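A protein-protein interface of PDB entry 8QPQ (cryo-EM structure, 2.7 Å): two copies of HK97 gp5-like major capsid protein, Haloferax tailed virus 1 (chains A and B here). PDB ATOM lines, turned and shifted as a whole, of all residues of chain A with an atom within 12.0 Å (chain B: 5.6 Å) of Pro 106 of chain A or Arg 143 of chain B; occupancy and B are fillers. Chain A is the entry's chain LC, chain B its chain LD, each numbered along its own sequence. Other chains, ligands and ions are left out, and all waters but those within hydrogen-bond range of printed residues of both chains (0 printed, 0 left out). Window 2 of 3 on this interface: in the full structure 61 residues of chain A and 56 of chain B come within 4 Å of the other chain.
Printed residues of chain B that touch a printed residue of chain A: Ala 140, Asn 141, Thr 142, Arg 143, Val 144, Gly 145 and Trp 177. Hydrophobic or aromatic side chains of chain B within 4 Å of the printed part of chain A: Ala 140, Val 144 and Trp 177. Of the 18 printed residues of chain A, 5 touch a printed residue of chain B. Among the printed residues, 11 pairs touch across the chains.
NH1 of Arg 143 of chain B sits close to ND2 of Asn 178 of chain B, 3.5 Å away. The backbone carbonyl oxygen of Arg 143 of chain B lies within hydrogen-bond range of the backbone NH of Ala 179 of chain B, 2.8 Å away. NE1 of Trp 177 of chain B is in hydrogen-bond range of O of Thr 142 of chain B (3.0 Å). The guanidinium group (NH2) of Arg 114 of chain A lies within salt-bridge range of the side-chain carboxylate (OD1) of Asp 110 of chain A (2.8 Å). The backbone carbonyl oxygen (O) of Val 144 of chain B lies within hydrogen-bond range of the side-chain hydroxyl (OG1) of Thr 142 of chain B, 2.6 Å away. The backbone NH of Trp 177 of chain B sits at hydrogen-bond distance from the backbone carbonyl oxygen of Gly 145 of chain B, 2.8 Å away.
Printed residues of chain B within 4 Å of Asp 105 of chain A: Arg 143 (2.5 Å). Pro 106 of chain A touches just one residue of chain B: Arg 143. Of the printed residues of chain B, Arg 114 of chain A touches Thr 142 (3.7 Å). Printed residues of chain B within 4 Å of Glu 115 of chain A: Thr 142 (3.9 Å) and Val 144 (3.4 Å). Of chain A, only Gln 116 comes within 4 Å of Ala 140 of chain B. Of the printed residues of chain A, Asn 141 of chain B touches Gln 116 (2.9 Å). Of chain A, only Arg 114 (3.7 Å), Glu 115 (3.9 Å) and Gln 116 (2.9 Å) come within 4 Å of Thr 142 of chain B. Of the printed residues of chain A, Arg 143 of chain B touches Asp 105 (2.5 Å) and Pro 106 (3.9 Å). Printed residues of chain A within 4 Å of Trp 177 of chain B: Gln 116 (3.3 Å). Asn 178 of chain B touches none of the printed residues of chain A. No residue of chain A comes within 4 Å of Ala 179 of chain B. No residue of chain A comes within 4 Å of Thr 180 of chain B. No residue of chain A comes within 4 Å of Tyr 353 of chain B. The nearest residue of chain A that does not touch Arg 143 of chain B is Val 109 of chain A (5.2 Å).
No position is printed for both chains. Of the 11 pairs that touch across the chains among the printed residues, none has its exchanged pair printed and touching as well.
The guanidinium group of Arg 143 of chain B is in salt-bridge range of the side-chain carboxylate of Asp 105 of chain A (2.5 Å). The backbone carbonyl oxygen (O) of Val 144 of chain B is in hydrogen-bond range of the backbone NH (N) of Gln 116 of chain A. The side-chain hydroxyl (OG1) of Thr 142 of chain B sits at hydrogen-bond distance from the backbone NH (N) of Gln 116 of chain A, at 2.9 Å. The side-chain amide oxygen (OE1) of Gln 116 of chain A sits at hydrogen-bond distance from the backbone NH (N) of Asn 141 of chain B (2.9 Å).
Pro 106 of chain A touches Arg 143 of chain B (CG to NH2, 3.9 Å). Arg 114 of chain A touches Thr 142 of chain B (O to CG2, 3.7 Å). Glu 115 of chain A touches Thr 142 of chain B. CD of Glu 115 of chain A touches CG1 of Val 144 of chain B, 3.4 Å away. CA of Ala 140 of chain B touches OE1 of Gln 116 of chain A, at 3.5 Å. Gln 116 of chain A touches Gly 145 of chain B (O to CA, 3.1 Å). Gln 116 of chain A touches Trp 177 of chain B (OE1 to CZ2, 3.3 Å).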
ATOM      1  N   PHE A 101     -10.555   1.281   4.784  1.00  0.00           N
ATOM      2  CA  PHE A 101     -10.785   1.111   6.255  1.00  0.00           C
ATOM      3  C   PHE A 101     -10.338   2.400   6.940  1.00  0.00           C
ATOM      4  O   PHE A 101     -11.038   3.400   6.860  1.00  0.00           O
ATOM      5  CB  PHE A 101     -10.182  -0.202   6.791  1.00  0.00           C
ATOM      6  CG  PHE A 101      -8.674  -0.386   6.761  1.00  0.00           C
ATOM      7  CD1 PHE A 101      -7.965  -0.434   5.564  1.00  0.00           C
ATOM      8  CD2 PHE A 101      -7.959  -0.532   7.949  1.00  0.00           C
ATOM      9  CE1 PHE A 101      -6.586  -0.600   5.557  1.00  0.00           C
ATOM     10  CE2 PHE A 101      -6.578  -0.689   7.938  1.00  0.00           C
ATOM     11  CZ  PHE A 101      -5.893  -0.715   6.740  1.00  0.00           C
ATOM     12  N   ALA A 102      -9.156   2.401   7.560  1.00  0.00           N
ATOM     13  CA  ALA A 102      -8.347   3.597   7.727  1.00  0.00           C
ATOM     14  C   ALA A 102      -7.792   3.981   6.351  1.00  0.00           C
ATOM     15  O   ALA A 102      -8.168   3.397   5.338  1.00  0.00           O
ATOM     16  CB  ALA A 102      -7.259   3.273   8.735  1.00  0.00           C
ATOM     17  N   ALA A 103      -6.857   4.947   6.315  1.00  0.00           N
ATOM     18  CA  ALA A 103      -6.058   5.211   5.125  1.00  0.00           C
ATOM     19  C   ALA A 103      -4.834   4.282   5.171  1.00  0.00           C
ATOM     20  O   ALA A 103      -4.028   4.316   6.110  1.00  0.00           O
ATOM     21  CB  ALA A 103      -5.675   6.676   5.086  1.00  0.00           C
ATOM     22  N   SER A 104      -4.658   3.503   4.090  1.00  0.00           N
ATOM     23  CA  SER A 104      -3.480   2.679   3.872  1.00  0.00           C
ATOM     24  C   SER A 104      -2.810   3.040   2.532  1.00  0.00           C
ATOM     25  O   SER A 104      -3.477   3.476   1.597  1.00  0.00           O
ATOM     26  CB  SER A 104      -3.853   1.212   3.968  1.00  0.00           C
ATOM     27  OG  SER A 104      -4.686   0.821   2.863  1.00  0.00           O
ATOM     28  N   ASP A 105      -1.501   2.760   2.444  1.00  0.00           N
ATOM     29  CA  ASP A 105      -0.730   3.081   1.256  1.00  0.00           C
ATOM     30  C   ASP A 105      -1.269   2.427  -0.009  1.00  0.00           C
ATOM     31  O   ASP A 105      -1.313   3.130  -1.015  1.00  0.00           O
ATOM     32  CB  ASP A 105       0.775   3.091   1.507  1.00  0.00           C
ATOM     33  CG  ASP A 105       1.480   1.756   1.395  1.00  0.00           C
ATOM     34  OD1 ASP A 105       1.456   1.178   0.306  1.00  0.00           O
ATOM     35  OD2 ASP A 105       2.176   1.356   2.371  1.00  0.00           O
ATOM     36  N   PRO A 106      -1.718   1.148  -0.054  1.00  0.00           N
ATOM     37  CA  PRO A 106      -2.253   0.547  -1.268  1.00  0.00           C
ATOM     38  C   PRO A 106      -3.459   1.237  -1.887  1.00  0.00           C
ATOM     39  O   PRO A 106      -3.657   1.119  -3.093  1.00  0.00           O
ATOM     40  CB  PRO A 106      -2.593  -0.903  -0.899  1.00  0.00           C
ATOM     41  CG  PRO A 106      -1.755  -1.186   0.313  1.00  0.00           C
ATOM     42  CD  PRO A 106      -1.649   0.148   1.010  1.00  0.00           C
ATOM     43  N   GLU A 107      -4.189   2.031  -1.100  1.00  0.00           N
ATOM     44  CA  GLU A 107      -5.321   2.803  -1.614  1.00  0.00           C
ATOM     45  C   GLU A 107      -4.882   4.091  -2.315  1.00  0.00           C
ATOM     46  O   GLU A 107      -5.557   4.557  -3.227  1.00  0.00           O
ATOM     47  CB  GLU A 107      -6.258   3.176  -0.468  1.00  0.00           C
ATOM     48  CG  GLU A 107      -6.831   1.981   0.263  1.00  0.00           C
ATOM     49  CD  GLU A 107      -7.453   2.387   1.572  1.00  0.00           C
ATOM     50  OE1 GLU A 107      -8.594   2.844   1.517  1.00  0.00           O
ATOM     51  OE2 GLU A 107      -6.742   2.361   2.596  1.00  0.00           O
ATOM     52  N   TYR A 108      -3.757   4.680  -1.890  1.00  0.00           N
ATOM     53  CA  TYR A 108      -3.370   6.042  -2.236  1.00  0.00           C
ATOM     54  C   TYR A 108      -1.992   6.140  -2.898  1.00  0.00           C
ATOM     55  O   TYR A 108      -1.455   7.253  -2.998  1.00  0.00           O
ATOM     56  CB  TYR A 108      -3.528   6.967  -1.021  1.00  0.00           C
ATOM     57  CG  TYR A 108      -4.932   6.996  -0.460  1.00  0.00           C
ATOM     58  CD1 TYR A 108      -6.030   7.269  -1.270  1.00  0.00           C
ATOM     59  CD2 TYR A 108      -5.170   6.747   0.881  1.00  0.00           C
ATOM     60  CE1 TYR A 108      -7.319   7.259  -0.767  1.00  0.00           C
ATOM     61  CE2 TYR A 108      -6.451   6.760   1.422  1.00  0.00           C
ATOM     62  CZ  TYR A 108      -7.530   7.034   0.588  1.00  0.00           C
ATOM     63  OH  TYR A 108      -8.803   7.052   1.091  1.00  0.00           O
ATOM     64  N   VAL A 109      -1.491   5.019  -3.451  1.00  0.00           N
ATOM     65  CA  VAL A 109      -0.204   4.867  -4.131  1.00  0.00           C
ATOM     66  C   VAL A 109       0.049   5.869  -5.276  1.00  0.00           C
ATOM     67  O   VAL A 109       1.211   6.079  -5.635  1.00  0.00           O
ATOM     68  CB  VAL A 109      -0.031   3.437  -4.706  1.00  0.00           C
ATOM     69  CG1 VAL A 109       0.039   2.369  -3.672  1.00  0.00           C
ATOM     70  CG2 VAL A 109      -1.020   3.089  -5.808  1.00  0.00           C
ATOM     71  N   ASP A 110      -1.010   6.444  -5.880  1.00  0.00           N
ATOM     72  CA  ASP A 110      -0.882   7.404  -6.957  1.00  0.00           C
ATOM     73  C   ASP A 110      -1.698   8.676  -6.693  1.00  0.00           C
ATOM     74  O   ASP A 110      -1.858   9.503  -7.605  1.00  0.00           O
ATOM     75  CB  ASP A 110      -1.215   6.762  -8.309  1.00  0.00           C
ATOM     76  CG  ASP A 110      -0.002   6.365  -9.152  1.00  0.00           C
ATOM     77  OD1 ASP A 110       0.969   7.172  -9.248  1.00  0.00           O
ATOM     78  OD2 ASP A 110      -0.060   5.287  -9.770  1.00  0.00           O
ATOM     79  N   THR A 111      -2.215   8.850  -5.460  1.00  0.00           N
ATOM     80  CA  THR A 111      -3.010  10.032  -5.130  1.00  0.00           C
ATOM     81  C   THR A 111      -2.291  10.923  -4.117  1.00  0.00           C
ATOM     82  O   THR A 111      -2.184  12.123  -4.345  1.00  0.00           O
ATOM     83  CB  THR A 111      -4.460   9.706  -4.743  1.00  0.00           C
ATOM     84  OG1 THR A 111      -4.464   9.174  -3.428  1.00  0.00           O
ATOM     85  CG2 THR A 111      -5.123   8.741  -5.700  1.00  0.00           C
ATOM     86  N   LEU A 112      -1.743  10.327  -3.045  1.00  0.00           N
ATOM     87  CA  LEU A 112      -1.074  11.087  -1.989  1.00  0.00           C
ATOM     88  C   LEU A 112       0.454  11.068  -2.100  1.00  0.00           C
ATOM     89  O   LEU A 112       1.119  11.889  -1.468  1.00  0.00           O
ATOM     90  CB  LEU A 112      -1.520  10.550  -0.628  1.00  0.00           C
ATOM     91  CG  LEU A 112      -2.985  10.787  -0.275  1.00  0.00           C
ATOM     92  CD1 LEU A 112      -3.289  10.187   1.083  1.00  0.00           C
ATOM     93  CD2 LEU A 112      -3.311  12.275  -0.284  1.00  0.00           C
ATOM     94  N   PHE A 113       0.996  10.135  -2.897  1.00  0.00           N
ATOM     95  CA  PHE A 113       2.423  10.028  -3.171  1.00  0.00           C
ATOM     96  C   PHE A 113       2.624   9.368  -4.538  1.00  0.00           C
ATOM     97  O   PHE A 113       1.657   8.940  -5.157  1.00  0.00           O
ATOM     98  CB  PHE A 113       3.135   9.297  -2.027  1.00  0.00           C
ATOM     99  CG  PHE A 113       2.743   7.853  -1.821  1.00  0.00           C
ATOM    100  CD1 PHE A 113       1.612   7.492  -1.090  1.00  0.00           C
ATOM    101  CD2 PHE A 113       3.530   6.838  -2.344  1.00  0.00           C
ATOM    102  CE1 PHE A 113       1.290   6.152  -0.890  1.00  0.00           C
ATOM    103  CE2 PHE A 113       3.200   5.501  -2.166  1.00  0.00           C
ATOM    104  CZ  PHE A 113       2.084   5.167  -1.436  1.00  0.00           C
ATOM    105  N   ARG A 114       3.875   9.319  -5.018  1.00  0.00           N
ATOM    106  CA  ARG A 114       4.260   8.558  -6.201  1.00  0.00           C
ATOM    107  C   ARG A 114       5.222   7.443  -5.789  1.00  0.00           C
ATOM    108  O   ARG A 114       6.071   7.645  -4.918  1.00  0.00           O
ATOM    109  CB  ARG A 114       4.958   9.463  -7.227  1.00  0.00           C
ATOM    110  CG  ARG A 114       4.062  10.477  -7.926  1.00  0.00           C
ATOM    111  CD  ARG A 114       3.040   9.843  -8.858  1.00  0.00           C
ATOM    112  NE  ARG A 114       2.431  10.875  -9.673  1.00  0.00           N
ATOM    113  CZ  ARG A 114       1.278  10.790 -10.317  1.00  0.00           C
ATOM    114  NH1 ARG A 114       0.851  11.829 -11.010  1.00  0.00           N
ATOM    115  NH2 ARG A 114       0.562   9.686 -10.296  1.00  0.00           N
ATOM    116  N   GLU A 115       5.095   6.259  -6.409  1.00  0.00           N
ATOM    117  CA  GLU A 115       6.092   5.201  -6.290  1.00  0.00           C
ATOM    118  C   GLU A 115       7.484   5.758  -6.613  1.00  0.00           C
ATOM    119  O   GLU A 115       7.647   6.517  -7.575  1.00  0.00           O
ATOM    120  CB  GLU A 115       5.762   4.057  -7.257  1.00  0.00           C
ATOM    121  CG  GLU A 115       4.621   3.152  -6.830  1.00  0.00           C
ATOM    122  CD  GLU A 115       4.176   2.140  -7.880  1.00  0.00           C
ATOM    123  OE1 GLU A 115       4.985   1.784  -8.765  1.00  0.00           O
ATOM    124  OE2 GLU A 115       3.016   1.693  -7.805  1.00  0.00           O
ATOM    125  N   GLN A 116       8.493   5.364  -5.821  1.00  0.00           N
ATOM    126  CA  GLN A 116       9.865   5.783  -6.077  1.00  0.00           C
ATOM    127  C   GLN A 116      10.385   5.179  -7.382  1.00  0.00           C
ATOM    128  O   GLN A 116      10.221   3.987  -7.635  1.00  0.00           O
ATOM    129  CB  GLN A 116      10.743   5.376  -4.900  1.00  0.00           C
ATOM    130  CG  GLN A 116      12.222   5.713  -5.060  1.00  0.00           C
ATOM    131  CD  GLN A 116      13.091   5.215  -3.924  1.00  0.00           C
ATOM    132  OE1 GLN A 116      12.666   4.443  -3.063  1.00  0.00           O
ATOM    133  NE2 GLN A 116      14.340   5.661  -3.907  1.00  0.00           N
ATOM    134  N   LEU A 117      10.987   6.024  -8.225  1.00  0.00           N
ATOM    135  CA  LEU A 117      11.783   5.575  -9.356  1.00  0.00           C
ATOM    136  C   LEU A 117      13.239   5.850  -9.001  1.00  0.00           C
ATOM    137  O   LEU A 117      13.567   6.985  -8.646  1.00  0.00           O
ATOM    138  CB  LEU A 117      11.350   6.343 -10.618  1.00  0.00           C
ATOM    139  CG  LEU A 117      11.864   5.805 -11.941  1.00  0.00           C
ATOM    140  CD1 LEU A 117      11.208   4.472 -12.291  1.00  0.00           C
ATOM    141  CD2 LEU A 117      11.586   6.816 -13.034  1.00  0.00           C
ATOM    142  N   LEU A 118      14.100   4.833  -9.118  1.00  0.00           N
ATOM    143  CA  LEU A 118      15.525   5.035  -8.915  1.00  0.00           C
ATOM    144  C   LEU A 118      16.088   5.832 -10.091  1.00  0.00           C
ATOM    145  O   LEU A 118      15.819   5.526 -11.250  1.00  0.00           O
ATOM    146  CB  LEU A 118      16.221   3.670  -8.855  1.00  0.00           C
ATOM    147  CG  LEU A 118      15.963   2.822  -7.611  1.00  0.00           C
ATOM    148  CD1 LEU A 118      16.974   1.697  -7.527  1.00  0.00           C
ATOM    149  CD2 LEU A 118      16.015   3.662  -6.346  1.00  0.00           C
ATOM    150  N   ALA B 140      14.643   1.979   0.529  1.00  0.00           N
ATOM    151  CA  ALA B 140      13.625   2.656  -0.262  1.00  0.00           C
ATOM    152  C   ALA B 140      12.944   3.778   0.524  1.00  0.00           C
ATOM    153  O   ALA B 140      12.755   3.693   1.738  1.00  0.00           O
ATOM    154  CB  ALA B 140      12.627   1.640  -0.722  1.00  0.00           C
ATOM    155  N   ASN B 141      12.519   4.816  -0.200  1.00  0.00           N
ATOM    156  CA  ASN B 141      11.682   5.875   0.349  1.00  0.00           C
ATOM    157  C   ASN B 141      10.195   5.495   0.344  1.00  0.00           C
ATOM    158  O   ASN B 141       9.427   6.030   1.136  1.00  0.00           O
ATOM    159  CB  ASN B 141      11.911   7.194  -0.373  1.00  0.00           C
ATOM    160  CG  ASN B 141      13.318   7.720  -0.173  1.00  0.00           C
ATOM    161  OD1 ASN B 141      14.233   7.393  -0.924  1.00  0.00           O
ATOM    162  ND2 ASN B 141      13.497   8.560   0.834  1.00  0.00           N
ATOM    163  N   THR B 142       9.807   4.577  -0.552  1.00  0.00           N
ATOM    164  CA  THR B 142       8.429   4.108  -0.685  1.00  0.00           C
ATOM    165  C   THR B 142       8.381   2.583  -0.699  1.00  0.00           C
ATOM    166  O   THR B 142       9.249   1.926  -1.263  1.00  0.00           O
ATOM    167  CB  THR B 142       7.695   4.711  -1.889  1.00  0.00           C
ATOM    168  OG1 THR B 142       8.389   4.388  -3.089  1.00  0.00           O
ATOM    169  CG2 THR B 142       7.517   6.210  -1.785  1.00  0.00           C
ATOM    170  N   ARG B 143       7.291   2.027  -0.146  1.00  0.00           N
ATOM    171  CA  ARG B 143       7.062   0.593  -0.071  1.00  0.00           C
ATOM    172  C   ARG B 143       6.924  -0.026  -1.464  1.00  0.00           C
ATOM    173  O   ARG B 143       7.292  -1.185  -1.669  1.00  0.00           O
ATOM    174  CB  ARG B 143       5.800   0.381   0.761  1.00  0.00           C
ATOM    175  CG  ARG B 143       5.508  -1.064   1.135  1.00  0.00           C
ATOM    176  CD  ARG B 143       4.057  -1.219   1.565  1.00  0.00           C
ATOM    177  NE  ARG B 143       3.470  -2.355   0.876  1.00  0.00           N
ATOM    178  CZ  ARG B 143       2.585  -2.303  -0.098  1.00  0.00           C
ATOM    179  NH1 ARG B 143       2.194  -3.436  -0.658  1.00  0.00           N
ATOM    180  NH2 ARG B 143       2.067  -1.152  -0.479  1.00  0.00           N
ATOM    181  N   VAL B 144       6.405   0.752  -2.421  1.00  0.00           N
ATOM    182  CA  VAL B 144       6.289   0.326  -3.812  1.00  0.00           C
ATOM    183  C   VAL B 144       7.148   1.253  -4.668  1.00  0.00           C
ATOM    184  O   VAL B 144       7.185   2.454  -4.433  1.00  0.00           O
ATOM    185  CB  VAL B 144       4.819   0.289  -4.282  1.00  0.00           C
ATOM    186  CG1 VAL B 144       4.690  -0.403  -5.617  1.00  0.00           C
ATOM    187  CG2 VAL B 144       3.909  -0.384  -3.270  1.00  0.00           C
ATOM    188  N   GLY B 145       7.848   0.690  -5.654  1.00  0.00           N
ATOM    189  CA  GLY B 145       8.730   1.466  -6.495  1.00  0.00           C
ATOM    190  C   GLY B 145       9.199   0.697  -7.715  1.00  0.00           C
ATOM    191  O   GLY B 145       8.883  -0.463  -7.878  1.00  0.00           O
ATOM    192  N   TRP B 177       9.347  -3.175  -7.267  1.00  0.00           N
ATOM    193  CA  TRP B 177       9.334  -3.728  -5.921  1.00  0.00           C
ATOM    194  C   TRP B 177       8.009  -3.396  -5.241  1.00  0.00           C
ATOM    195  O   TRP B 177       7.490  -2.312  -5.416  1.00  0.00           O
ATOM    196  CB  TRP B 177      10.554  -3.277  -5.105  1.00  0.00           C
ATOM    197  CG  TRP B 177      10.566  -1.873  -4.560  1.00  0.00           C
ATOM    198  CD1 TRP B 177       9.952  -1.423  -3.424  1.00  0.00           C
ATOM    199  CD2 TRP B 177      11.298  -0.735  -5.082  1.00  0.00           C
ATOM    200  NE1 TRP B 177      10.246  -0.105  -3.217  1.00  0.00           N
ATOM    201  CE2 TRP B 177      11.097   0.348  -4.193  1.00  0.00           C
ATOM    202  CE3 TRP B 177      12.107  -0.513  -6.205  1.00  0.00           C
ATOM    203  CZ2 TRP B 177      11.689   1.611  -4.392  1.00  0.00           C
ATOM    204  CZ3 TRP B 177      12.681   0.732  -6.413  1.00  0.00           C
ATOM    205  CH2 TRP B 177      12.488   1.779  -5.506  1.00  0.00           C
ATOM    206  N   ASN B 178       7.478  -4.337  -4.473  1.00  0.00           N
ATOM    207  CA  ASN B 178       6.432  -4.050  -3.507  1.00  0.00           C
ATOM    208  C   ASN B 178       6.776  -4.743  -2.193  1.00  0.00           C
ATOM    209  O   ASN B 178       6.643  -5.951  -2.063  1.00  0.00           O
ATOM    210  CB  ASN B 178       4.988  -4.130  -4.052  1.00  0.00           C
ATOM    211  CG  ASN B 178       4.328  -5.483  -3.984  1.00  0.00           C
ATOM    212  OD1 ASN B 178       4.763  -6.406  -4.651  1.00  0.00           O
ATOM    213  ND2 ASN B 178       3.366  -5.626  -3.084  1.00  0.00           N
ATOM    214  N   ALA B 179       7.309  -3.974  -1.258  1.00  0.00           N
ATOM    215  CA  ALA B 179       7.821  -4.477   0.002  1.00  0.00           C
ATOM    216  C   ALA B 179       6.696  -5.038   0.867  1.00  0.00           C
ATOM    217  O   ALA B 179       5.682  -4.389   1.080  1.00  0.00           O
ATOM    218  CB  ALA B 179       8.646  -3.397   0.659  1.00  0.00           C
ATOM    219  N   THR B 180       6.867  -6.282   1.319  1.00  0.00           N
ATOM    220  CA  THR B 180       5.894  -6.962   2.160  1.00  0.00           C
ATOM    221  C   THR B 180       6.260  -6.723   3.622  1.00  0.00           C
ATOM    222  O   THR B 180       7.424  -6.859   3.988  1.00  0.00           O
ATOM    223  CB  THR B 180       5.900  -8.466   1.851  1.00  0.00           C
ATOM    224  OG1 THR B 180       5.455  -8.653   0.509  1.00  0.00           O
ATOM    225  CG2 THR B 180       4.996  -9.289   2.743  1.00  0.00           C
ATOM    226  N   TYR B 353      12.143  -1.165   3.333  1.00  0.00           N
ATOM    227  CA  TYR B 353      11.359   0.007   3.678  1.00  0.00           C
ATOM    228  C   TYR B 353      10.958  -0.049   5.154  1.00  0.00           C
ATOM    229  O   TYR B 353      10.517  -1.076   5.669  1.00  0.00           O
ATOM    230  CB  TYR B 353      10.161   0.141   2.727  1.00  0.00           C
ATOM    231  CG  TYR B 353       9.197   1.229   3.131  1.00  0.00           C
ATOM    232  CD1 TYR B 353       9.514   2.572   2.957  1.00  0.00           C
ATOM    233  CD2 TYR B 353       7.986   0.915   3.734  1.00  0.00           C
ATOM    234  CE1 TYR B 353       8.655   3.575   3.383  1.00  0.00           C
ATOM    235  CE2 TYR B 353       7.108   1.911   4.143  1.00  0.00           C
ATOM    236  CZ  TYR B 353       7.444   3.245   3.973  1.00  0.00           C
ATOM    237  OH  TYR B 353       6.599   4.228   4.403  1.00  0.00           O
ATOM    238  N   HIS B 380       9.566  -3.811   6.208  1.00  0.00           N
ATOM    239  CA  HIS B 380       9.025  -4.157   4.904  1.00  0.00           C
ATOM    240  C   HIS B 380      10.186  -4.530   3.992  1.00  0.00           C
ATOM    241  O   HIS B 380      11.174  -3.795   3.888  1.00  0.00           O
ATOM    242  CB  HIS B 380       8.194  -3.011   4.306  1.00  0.00           C
ATOM    243  CG  HIS B 380       7.080  -2.529   5.161  1.00  0.00           C
ATOM    244  ND1 HIS B 380       5.746  -2.606   4.805  1.00  0.00           N
ATOM    245  CD2 HIS B 380       7.130  -1.832   6.307  1.00  0.00           C
ATOM    246  CE1 HIS B 380       5.022  -1.998   5.716  1.00  0.00           C
ATOM    247  NE2 HIS B 380       5.848  -1.540   6.659  1.00  0.00           N
